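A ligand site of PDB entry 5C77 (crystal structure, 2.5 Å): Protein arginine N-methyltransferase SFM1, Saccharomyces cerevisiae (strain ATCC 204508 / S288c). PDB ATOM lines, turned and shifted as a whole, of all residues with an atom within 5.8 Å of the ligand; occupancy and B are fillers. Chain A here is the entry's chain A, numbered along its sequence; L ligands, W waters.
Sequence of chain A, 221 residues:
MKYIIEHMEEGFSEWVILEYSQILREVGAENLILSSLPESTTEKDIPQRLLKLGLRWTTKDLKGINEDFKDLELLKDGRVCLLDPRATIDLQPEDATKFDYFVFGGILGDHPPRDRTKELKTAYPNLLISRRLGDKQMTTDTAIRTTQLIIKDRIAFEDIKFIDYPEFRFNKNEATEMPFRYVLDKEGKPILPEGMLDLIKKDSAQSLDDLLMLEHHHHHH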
ATOM      1  N   MET A   8      10.196 -14.566  -1.086  1.00  0.00           N
ATOM      2  CA  MET A   8       9.929 -15.744  -0.241  1.00  0.00           C
ATOM      3  C   MET A   8      11.145 -16.535   0.252  1.00  0.00           C
ATOM      4  O   MET A   8      11.089 -17.764   0.362  1.00  0.00           O
ATOM      5  CB  MET A   8       8.983 -16.720  -0.953  1.00  0.00           C
ATOM      6  CG  MET A   8       7.492 -16.365  -0.898  1.00  0.00           C
ATOM      7  SD  MET A   8       6.801 -16.110   0.764  1.00  0.00           S
ATOM      8  CE  MET A   8       6.931 -14.318   0.884  1.00  0.00           C
ATOM      9  N   GLU A   9      12.245 -15.845   0.536  1.00  0.00           N
ATOM     10  CA  GLU A   9      13.398 -16.505   1.134  1.00  0.00           C
ATOM     11  C   GLU A   9      14.349 -15.503   1.787  1.00  0.00           C
ATOM     12  O   GLU A   9      14.193 -14.302   1.627  1.00  0.00           O
ATOM     13  CB  GLU A   9      14.137 -17.395   0.126  1.00  0.00           C
ATOM     14  CG  GLU A   9      14.667 -16.688  -1.122  1.00  0.00           C
ATOM     15  CD  GLU A   9      15.375 -17.651  -2.078  1.00  0.00           C
ATOM     16  OE1 GLU A   9      16.620 -17.720  -2.033  1.00  0.00           O
ATOM     17  OE2 GLU A   9      14.676 -18.358  -2.842  1.00  0.00           O
ATOM     18  N   LEU A  83      -2.702 -14.367  -5.839  1.00  0.00           N
ATOM     19  CA  LEU A  83      -2.697 -15.698  -6.441  1.00  0.00           C
ATOM     20  C   LEU A  83      -2.334 -16.787  -5.441  1.00  0.00           C
ATOM     21  O   LEU A  83      -1.291 -16.731  -4.775  1.00  0.00           O
ATOM     22  CB  LEU A  83      -1.798 -15.697  -7.681  1.00  0.00           C
ATOM     23  CG  LEU A  83      -2.435 -14.760  -8.711  1.00  0.00           C
ATOM     24  CD1 LEU A  83      -1.431 -13.981  -9.508  1.00  0.00           C
ATOM     25  CD2 LEU A  83      -3.362 -15.555  -9.621  1.00  0.00           C
ATOM     26  N   ASP A  84      -3.221 -17.772  -5.322  1.00  0.00           N
ATOM     27  CA  ASP A  84      -3.129 -18.819  -4.304  1.00  0.00           C
ATOM     28  C   ASP A  84      -3.666 -20.126  -4.879  1.00  0.00           C
ATOM     29  O   ASP A  84      -4.797 -20.169  -5.347  1.00  0.00           O
ATOM     30  CB  ASP A  84      -3.939 -18.413  -3.076  1.00  0.00           C
ATOM     31  CG  ASP A  84      -4.085 -19.537  -2.063  1.00  0.00           C
ATOM     32  OD1 ASP A  84      -3.187 -20.399  -1.952  1.00  0.00           O
ATOM     33  OD2 ASP A  84      -5.098 -19.536  -1.337  1.00  0.00           O
ATOM     34  N   PRO A  85      -2.841 -21.188  -4.842  1.00  0.00           N
ATOM     35  CA  PRO A  85      -3.228 -22.505  -5.369  1.00  0.00           C
ATOM     36  C   PRO A  85      -4.362 -23.156  -4.570  1.00  0.00           C
ATOM     37  O   PRO A  85      -4.949 -24.129  -5.027  1.00  0.00           O
ATOM     38  CB  PRO A  85      -1.935 -23.316  -5.231  1.00  0.00           C
ATOM     39  CG  PRO A  85      -1.161 -22.618  -4.168  1.00  0.00           C
ATOM     40  CD  PRO A  85      -1.465 -21.183  -4.331  1.00  0.00           C
ATOM     41  N   ARG A  86      -4.672 -22.595  -3.402  1.00  0.00           N
ATOM     42  CA  ARG A  86      -5.747 -23.117  -2.567  1.00  0.00           C
ATOM     43  C   ARG A  86      -7.096 -22.431  -2.841  1.00  0.00           C
ATOM     44  O   ARG A  86      -8.144 -22.891  -2.364  1.00  0.00           O
ATOM     45  CB  ARG A  86      -5.350 -22.997  -1.094  1.00  0.00           C
ATOM     46  CG  ARG A  86      -6.328 -23.634  -0.114  1.00  0.00           C
ATOM     47  CD  ARG A  86      -5.976 -23.328   1.347  1.00  0.00           C
ATOM     48  NE  ARG A  86      -7.046 -23.727   2.250  1.00  0.00           N
ATOM     49  CZ  ARG A  86      -7.284 -24.983   2.627  1.00  0.00           C
ATOM     50  NH1 ARG A  86      -6.528 -25.966   2.161  1.00  0.00           N
ATOM     51  NH2 ARG A  86      -8.282 -25.249   3.475  1.00  0.00           N
ATOM     52  N   VAL A 103      -0.548 -10.349  -7.120  1.00  0.00           N
ATOM     53  CA  VAL A 103       0.363 -10.547  -6.001  1.00  0.00           C
ATOM     54  C   VAL A 103       0.692 -12.030  -5.805  1.00  0.00           C
ATOM     55  O   VAL A 103      -0.172 -12.906  -5.863  1.00  0.00           O
ATOM     56  CB  VAL A 103      -0.198  -9.925  -4.701  1.00  0.00           C
ATOM     57  CG1 VAL A 103       0.795 -10.060  -3.553  1.00  0.00           C
ATOM     58  CG2 VAL A 103      -0.532  -8.455  -4.933  1.00  0.00           C
ATOM     59  N   PHE A 104       1.974 -12.285  -5.578  1.00  0.00           N
ATOM     60  CA  PHE A 104       2.452 -13.627  -5.332  1.00  0.00           C
ATOM     61  C   PHE A 104       3.012 -13.684  -3.932  1.00  0.00           C
ATOM     62  O   PHE A 104       3.941 -12.942  -3.580  1.00  0.00           O
ATOM     63  CB  PHE A 104       3.490 -14.010  -6.387  1.00  0.00           C
ATOM     64  CG  PHE A 104       2.940 -13.979  -7.784  1.00  0.00           C
ATOM     65  CD1 PHE A 104       2.813 -12.788  -8.475  1.00  0.00           C
ATOM     66  CD2 PHE A 104       2.512 -15.139  -8.398  1.00  0.00           C
ATOM     67  CE1 PHE A 104       2.286 -12.750  -9.743  1.00  0.00           C
ATOM     68  CE2 PHE A 104       1.989 -15.115  -9.664  1.00  0.00           C
ATOM     69  CZ  PHE A 104       1.871 -13.919 -10.341  1.00  0.00           C
ATOM     70  N   GLY A 105       2.400 -14.550  -3.125  1.00  0.00           N
ATOM     71  CA  GLY A 105       2.825 -14.793  -1.749  1.00  0.00           C
ATOM     72  C   GLY A 105       3.604 -16.087  -1.690  1.00  0.00           C
ATOM     73  O   GLY A 105       4.541 -16.286  -2.462  1.00  0.00           O
ATOM     74  N   GLY A 106       3.203 -16.990  -0.793  1.00  0.00           N
ATOM     75  CA  GLY A 106       3.869 -18.272  -0.672  1.00  0.00           C
ATOM     76  C   GLY A 106       4.109 -18.692   0.776  1.00  0.00           C
ATOM     77  O   GLY A 106       3.422 -18.231   1.696  1.00  0.00           O
ATOM     78  N   ILE A 107       5.093 -19.568   0.973  1.00  0.00           N
ATOM     79  CA  ILE A 107       5.501 -19.995   2.299  1.00  0.00           C
ATOM     80  C   ILE A 107       6.953 -19.625   2.523  1.00  0.00           C
ATOM     81  O   ILE A 107       7.834 -20.059   1.787  1.00  0.00           O
ATOM     82  CB  ILE A 107       5.337 -21.524   2.497  1.00  0.00           C
ATOM     83  CG1 ILE A 107       3.882 -21.950   2.321  1.00  0.00           C
ATOM     84  CG2 ILE A 107       5.800 -21.934   3.876  1.00  0.00           C
ATOM     85  CD1 ILE A 107       3.641 -22.809   1.099  1.00  0.00           C
ATOM     86  N   LEU A 108       7.207 -18.807   3.543  1.00  0.00           N
ATOM     87  CA  LEU A 108       8.577 -18.397   3.843  1.00  0.00           C
ATOM     88  C   LEU A 108       9.259 -19.311   4.867  1.00  0.00           C
ATOM     89  O   LEU A 108       8.778 -19.485   6.004  1.00  0.00           O
ATOM     90  CB  LEU A 108       8.607 -16.935   4.294  1.00  0.00           C
ATOM     91  CG  LEU A 108       9.927 -16.423   4.866  1.00  0.00           C
ATOM     92  CD1 LEU A 108      11.011 -16.398   3.809  1.00  0.00           C
ATOM     93  CD2 LEU A 108       9.747 -15.048   5.480  1.00  0.00           C
ATOM     94  N   GLY A 109      10.380 -19.895   4.460  1.00  0.00           N
ATOM     95  CA  GLY A 109      11.195 -20.743   5.311  1.00  0.00           C
ATOM     96  C   GLY A 109      10.570 -22.077   5.678  1.00  0.00           C
ATOM     97  O   GLY A 109       9.607 -22.542   5.073  1.00  0.00           O
ATOM     98  N   THR A 117       0.828 -15.986   2.258  1.00  0.00           N
ATOM     99  CA  THR A 117      -0.435 -15.953   1.532  1.00  0.00           C
ATOM    100  C   THR A 117      -1.606 -15.689   2.473  1.00  0.00           C
ATOM    101  O   THR A 117      -2.449 -14.841   2.196  1.00  0.00           O
ATOM    102  CB  THR A 117      -0.679 -17.286   0.804  1.00  0.00           C
ATOM    103  OG1 THR A 117       0.334 -17.489  -0.183  1.00  0.00           O
ATOM    104  CG2 THR A 117      -2.022 -17.305   0.133  1.00  0.00           C
ATOM    105  N   ARG A 131      -7.416 -15.766  -6.408  1.00  0.00           N
ATOM    106  CA  ARG A 131      -7.645 -16.567  -7.626  1.00  0.00           C
ATOM    107  C   ARG A 131      -6.644 -17.714  -7.761  1.00  0.00           C
ATOM    108  O   ARG A 131      -5.506 -17.626  -7.311  1.00  0.00           O
ATOM    109  CB  ARG A 131      -7.606 -15.679  -8.863  1.00  0.00           C
ATOM    110  CG  ARG A 131      -8.775 -14.714  -8.961  1.00  0.00           C
ATOM    111  CD  ARG A 131     -10.031 -15.454  -9.403  1.00  0.00           C
ATOM    112  NE  ARG A 131     -11.202 -14.585  -9.408  1.00  0.00           N
ATOM    113  CZ  ARG A 131     -12.049 -14.464  -8.394  1.00  0.00           C
ATOM    114  NH1 ARG A 131     -11.861 -15.166  -7.283  1.00  0.00           N
ATOM    115  NH2 ARG A 131     -13.087 -13.657  -8.491  1.00  0.00           N
ATOM    116  N   ARG A 132      -7.077 -18.796  -8.403  1.00  0.00           N
ATOM    117  CA  ARG A 132      -6.237 -19.960  -8.591  1.00  0.00           C
ATOM    118  C   ARG A 132      -5.750 -20.029 -10.035  1.00  0.00           C
ATOM    119  O   ARG A 132      -6.360 -19.453 -10.941  1.00  0.00           O
ATOM    120  CB  ARG A 132      -6.994 -21.251  -8.238  1.00  0.00           C
ATOM    121  CG  ARG A 132      -6.097 -22.476  -8.061  1.00  0.00           C
ATOM    122  CD  ARG A 132      -6.873 -23.752  -7.860  1.00  0.00           C
ATOM    123  NE  ARG A 132      -7.634 -24.112  -9.049  1.00  0.00           N
ATOM    124  CZ  ARG A 132      -8.455 -25.163  -9.125  1.00  0.00           C
ATOM    125  NH1 ARG A 132      -8.612 -25.964  -8.090  1.00  0.00           N
ATOM    126  NH2 ARG A 132      -9.113 -25.404 -10.245  1.00  0.00           N
ATOM    127  N   LEU A 133      -4.634 -20.719 -10.227  1.00  0.00           N
ATOM    128  CA  LEU A 133      -4.068 -20.995 -11.541  1.00  0.00           C
ATOM    129  C   LEU A 133      -4.009 -22.503 -11.741  1.00  0.00           C
ATOM    130  O   LEU A 133      -2.935 -23.085 -11.838  1.00  0.00           O
ATOM    131  CB  LEU A 133      -2.657 -20.406 -11.666  1.00  0.00           C
ATOM    132  CG  LEU A 133      -2.598 -18.881 -11.623  1.00  0.00           C
ATOM    133  CD1 LEU A 133      -1.174 -18.372 -11.413  1.00  0.00           C
ATOM    134  CD2 LEU A 133      -3.209 -18.309 -12.905  1.00  0.00           C
ATOM    135  N   GLY A 134      -5.176 -23.130 -11.779  1.00  0.00           N
ATOM    136  CA  GLY A 134      -5.239 -24.569 -11.922  1.00  0.00           C
ATOM    137  C   GLY A 134      -4.924 -25.322 -10.648  1.00  0.00           C
ATOM    138  O   GLY A 134      -4.446 -24.738  -9.670  1.00  0.00           O
ATOM    139  N   ASP A 135      -5.170 -26.624 -10.667  1.00  0.00           N
ATOM    140  CA  ASP A 135      -5.111 -27.427  -9.451  1.00  0.00           C
ATOM    141  C   ASP A 135      -3.741 -28.024  -9.189  1.00  0.00           C
ATOM    142  O   ASP A 135      -3.588 -28.894  -8.331  1.00  0.00           O
ATOM    143  CB  ASP A 135      -6.174 -28.522  -9.493  1.00  0.00           C
ATOM    144  CG  ASP A 135      -5.935 -29.522 -10.588  1.00  0.00           C
ATOM    145  OD1 ASP A 135      -5.142 -29.208 -11.506  1.00  0.00           O
ATOM    146  OD2 ASP A 135      -6.534 -30.618 -10.544  1.00  0.00           O
ATOM    147  N   LYS A 136      -2.732 -27.567  -9.918  1.00  0.00           N
ATOM    148  CA  LYS A 136      -1.380 -28.026  -9.648  1.00  0.00           C
ATOM    149  C   LYS A 136      -0.479 -26.881  -9.245  1.00  0.00           C
ATOM    150  O   LYS A 136      -0.686 -25.746  -9.639  1.00  0.00           O
ATOM    151  CB  LYS A 136      -0.805 -28.791 -10.843  1.00  0.00           C
ATOM    152  CG  LYS A 136      -1.554 -30.079 -11.108  1.00  0.00           C
ATOM    153  CD  LYS A 136      -0.695 -31.111 -11.804  1.00  0.00           C
ATOM    154  CE  LYS A 136      -1.428 -32.436 -11.922  1.00  0.00           C
ATOM    155  NZ  LYS A 136      -1.913 -32.922 -10.589  1.00  0.00           N
ATOM    156  N   GLN A 137       0.515 -27.212  -8.444  1.00  0.00           N
ATOM    157  CA  GLN A 137       1.486 -26.250  -7.943  1.00  0.00           C
ATOM    158  C   GLN A 137       2.406 -25.812  -9.103  1.00  0.00           C
ATOM    159  O   GLN A 137       2.812 -26.632  -9.916  1.00  0.00           O
ATOM    160  CB  GLN A 137       2.272 -26.905  -6.804  1.00  0.00           C
ATOM    161  CG  GLN A 137       3.361 -26.052  -6.171  1.00  0.00           C
ATOM    162  CD  GLN A 137       2.806 -24.868  -5.400  1.00  0.00           C
ATOM    163  OE1 GLN A 137       1.825 -24.989  -4.662  1.00  0.00           O
ATOM    164  NE2 GLN A 137       3.438 -23.699  -5.575  1.00  0.00           N
ATOM    165  N   MET A 138       2.711 -24.518  -9.143  1.00  0.00           N
ATOM    166  CA  MET A 138       3.577 -23.949 -10.176  1.00  0.00           C
ATOM    167  C   MET A 138       4.739 -23.179  -9.559  1.00  0.00           C
ATOM    168  O   MET A 138       4.626 -22.653  -8.451  1.00  0.00           O
ATOM    169  CB  MET A 138       2.786 -22.959 -11.051  1.00  0.00           C
ATOM    170  CG  MET A 138       1.786 -23.573 -11.996  1.00  0.00           C
ATOM    171  SD  MET A 138       0.913 -22.311 -12.950  1.00  0.00           S
ATOM    172  CE  MET A 138       0.108 -23.316 -14.167  1.00  0.00           C
ATOM    173  N   THR A 139       5.855 -23.082 -10.271  1.00  0.00           N
ATOM    174  CA  THR A 139       6.919 -22.154  -9.895  1.00  0.00           C
ATOM    175  C   THR A 139       6.495 -20.699 -10.119  1.00  0.00           C
ATOM    176  O   THR A 139       5.534 -20.415 -10.835  1.00  0.00           O
ATOM    177  CB  THR A 139       8.206 -22.406 -10.701  1.00  0.00           C
ATOM    178  OG1 THR A 139       7.986 -22.083 -12.075  1.00  0.00           O
ATOM    179  CG2 THR A 139       8.669 -23.865 -10.581  1.00  0.00           C
ATOM    180  N   THR A 140       7.217 -19.768  -9.506  1.00  0.00           N
ATOM    181  CA  THR A 140       6.905 -18.345  -9.625  1.00  0.00           C
ATOM    182  C   THR A 140       6.912 -17.845 -11.068  1.00  0.00           C
ATOM    183  O   THR A 140       6.032 -17.083 -11.468  1.00  0.00           O
ATOM    184  CB  THR A 140       7.889 -17.488  -8.809  1.00  0.00           C
ATOM    185  OG1 THR A 140       8.295 -18.213  -7.651  1.00  0.00           O
ATOM    186  CG2 THR A 140       7.238 -16.167  -8.412  1.00  0.00           C
ATOM    187  N   ALA A 143       4.018 -19.383 -12.851  1.00  0.00           N
ATOM    188  CA  ALA A 143       2.779 -18.774 -12.384  1.00  0.00           C
ATOM    189  C   ALA A 143       2.612 -17.414 -13.064  1.00  0.00           C
ATOM    190  O   ALA A 143       1.520 -17.038 -13.485  1.00  0.00           O
ATOM    191  CB  ALA A 143       2.746 -18.649 -10.860  1.00  0.00           C
HETATM  192  N1  LIG L   1      10.136 -20.290  -1.959  1.00  0.00           N
HETATM  193  C1  LIG L   1       8.693 -20.102  -2.071  1.00  0.00           C
HETATM  194  C2  LIG L   1       8.243 -20.344  -3.523  1.00  0.00           C
HETATM  195  C3  LIG L   1       6.889 -19.722  -3.885  1.00  0.00           C
HETATM  196  S1  LIG L   1       6.331 -20.103  -5.576  1.00  0.00           S
HETATM  197  C4  LIG L   1       7.939 -21.007  -1.095  1.00  0.00           C
HETATM  198  O1  LIG L   1       6.710 -20.945  -0.981  1.00  0.00           O
HETATM  199  O2  LIG L   1       8.545 -21.816  -0.384  1.00  0.00           O
HETATM  200  C5  LIG L   1       4.629 -20.183  -4.961  1.00  0.00           C
HETATM  201  C6  LIG L   1       3.783 -19.007  -5.407  1.00  0.00           C
HETATM  202  O3  LIG L   1       3.438 -19.106  -6.785  1.00  0.00           O
HETATM  203  C7  LIG L   1       2.479 -18.973  -4.614  1.00  0.00           C
HETATM  204  O4  LIG L   1       2.565 -18.010  -3.597  1.00  0.00           O
HETATM  205  C8  LIG L   1       1.437 -18.543  -5.597  1.00  0.00           C
HETATM  206  O5  LIG L   1       1.335 -17.130  -5.579  1.00  0.00           O
HETATM  207  C9  LIG L   1       2.037 -18.944  -6.927  1.00  0.00           C
HETATM  208  N2  LIG L   1       1.397 -20.185  -7.387  1.00  0.00           N
HETATM  209  C10 LIG L   1       2.008 -21.389  -7.618  1.00  0.00           C
HETATM  210  N3  LIG L   1       1.079 -22.273  -8.030  1.00  0.00           N
HETATM  211  C11 LIG L   1      -0.118 -21.658  -8.059  1.00  0.00           C
HETATM  212  C12 LIG L   1      -1.406 -22.081  -8.401  1.00  0.00           C
HETATM  213  N4  LIG L   1      -1.630 -23.334  -8.799  1.00  0.00           N
HETATM  214  N5  LIG L   1      -2.453 -21.184  -8.335  1.00  0.00           N
HETATM  215  C13 LIG L   1      -2.246 -19.884  -7.934  1.00  0.00           C
HETATM  216  N6  LIG L   1      -0.983 -19.477  -7.586  1.00  0.00           N
HETATM  217  C14 LIG L   1       0.071 -20.335  -7.662  1.00  0.00           C
HETATM  218  O   HOH W   1      11.885 -18.539  -3.369  1.00  0.00           O
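The backbone NH (N) of Gly 106 sits at hydrogen-bond distance from an oxygen (O4) of the ligand (3.1 Å). O of Lys 136 is in hydrogen-bond range of N4 of the ligand (2.7 Å). O2 of the ligand sits close to O of Ile 107, at 2.9 Å. The backbone carbonyl oxygen of Leu 83 is in hydrogen-bond range of an oxygen (O5) of the ligand (2.8 Å). A nitrogen (N4) of the ligand lies within hydrogen-bond range of the backbone carbonyl oxygen (O) of Leu 133 (3.3 Å). A nitrogen (N3) of the ligand lies within hydrogen-bond range of the backbone NH of Met 138 (3.0 Å). The backbone NH (N) of Gly 105 sits close to an oxygen (O4) of the ligand (3.5 Å). An oxygen (O4) of the ligand sits at hydrogen-bond distance from the backbone carbonyl oxygen of Gly 105 (2.9 Å). N5 of the ligand sits at hydrogen-bond distance from N of Leu 133 (2.9 Å). O1 of the ligand sits at hydrogen-bond distance from N of Ile 107, 2.9 Å away. The side-chain hydroxyl (OG1) of Thr 140 lies close to a sulfur (S1) of the ligand, 3.4 Å away. O of Gly 134 lies within hydrogen-bond range of N4 of the ligand (3.3 Å).
The side-chain carboxylate (OD1) of Asp 84 is in hydrogen-bond range of the backbone NH (N) of Arg 86. The backbone NH (N) of Leu 83 sits at hydrogen-bond distance from the backbone carbonyl oxygen (O) of Val 103, 2.9 Å away. N of Asp 84 is in hydrogen-bond range of O of Arg 131, 3.0 Å away. The backbone carbonyl oxygen (O) of Gly 134 sits close to the guanidinium group (NE) of Arg 132, 3.3 Å away. The side-chain hydroxyl of Thr 117 is in hydrogen-bond range of the backbone NH of Gly 106 (3.0 Å).
Residues that only touch the ligand: Met 8 (3.6 Å), Asp 84 (3.4 Å), Pro 85 (3.3 Å), Phe 104 (3.6 Å), Arg 132 (3.9 Å) and Gln 137 (3.4 Å). Hydrophobic or aromatic side chains within 4 Å of the ligand: Met 8, Leu 83, Pro 85, Phe 104, Ile 107, Leu 133 and Met 138.
Water W1 lies within hydrogen-bond range of the side-chain carboxylate (OE2) of Glu 9 (2.8 Å) and a nitrogen (N1) of the ligand (2.8 Å).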
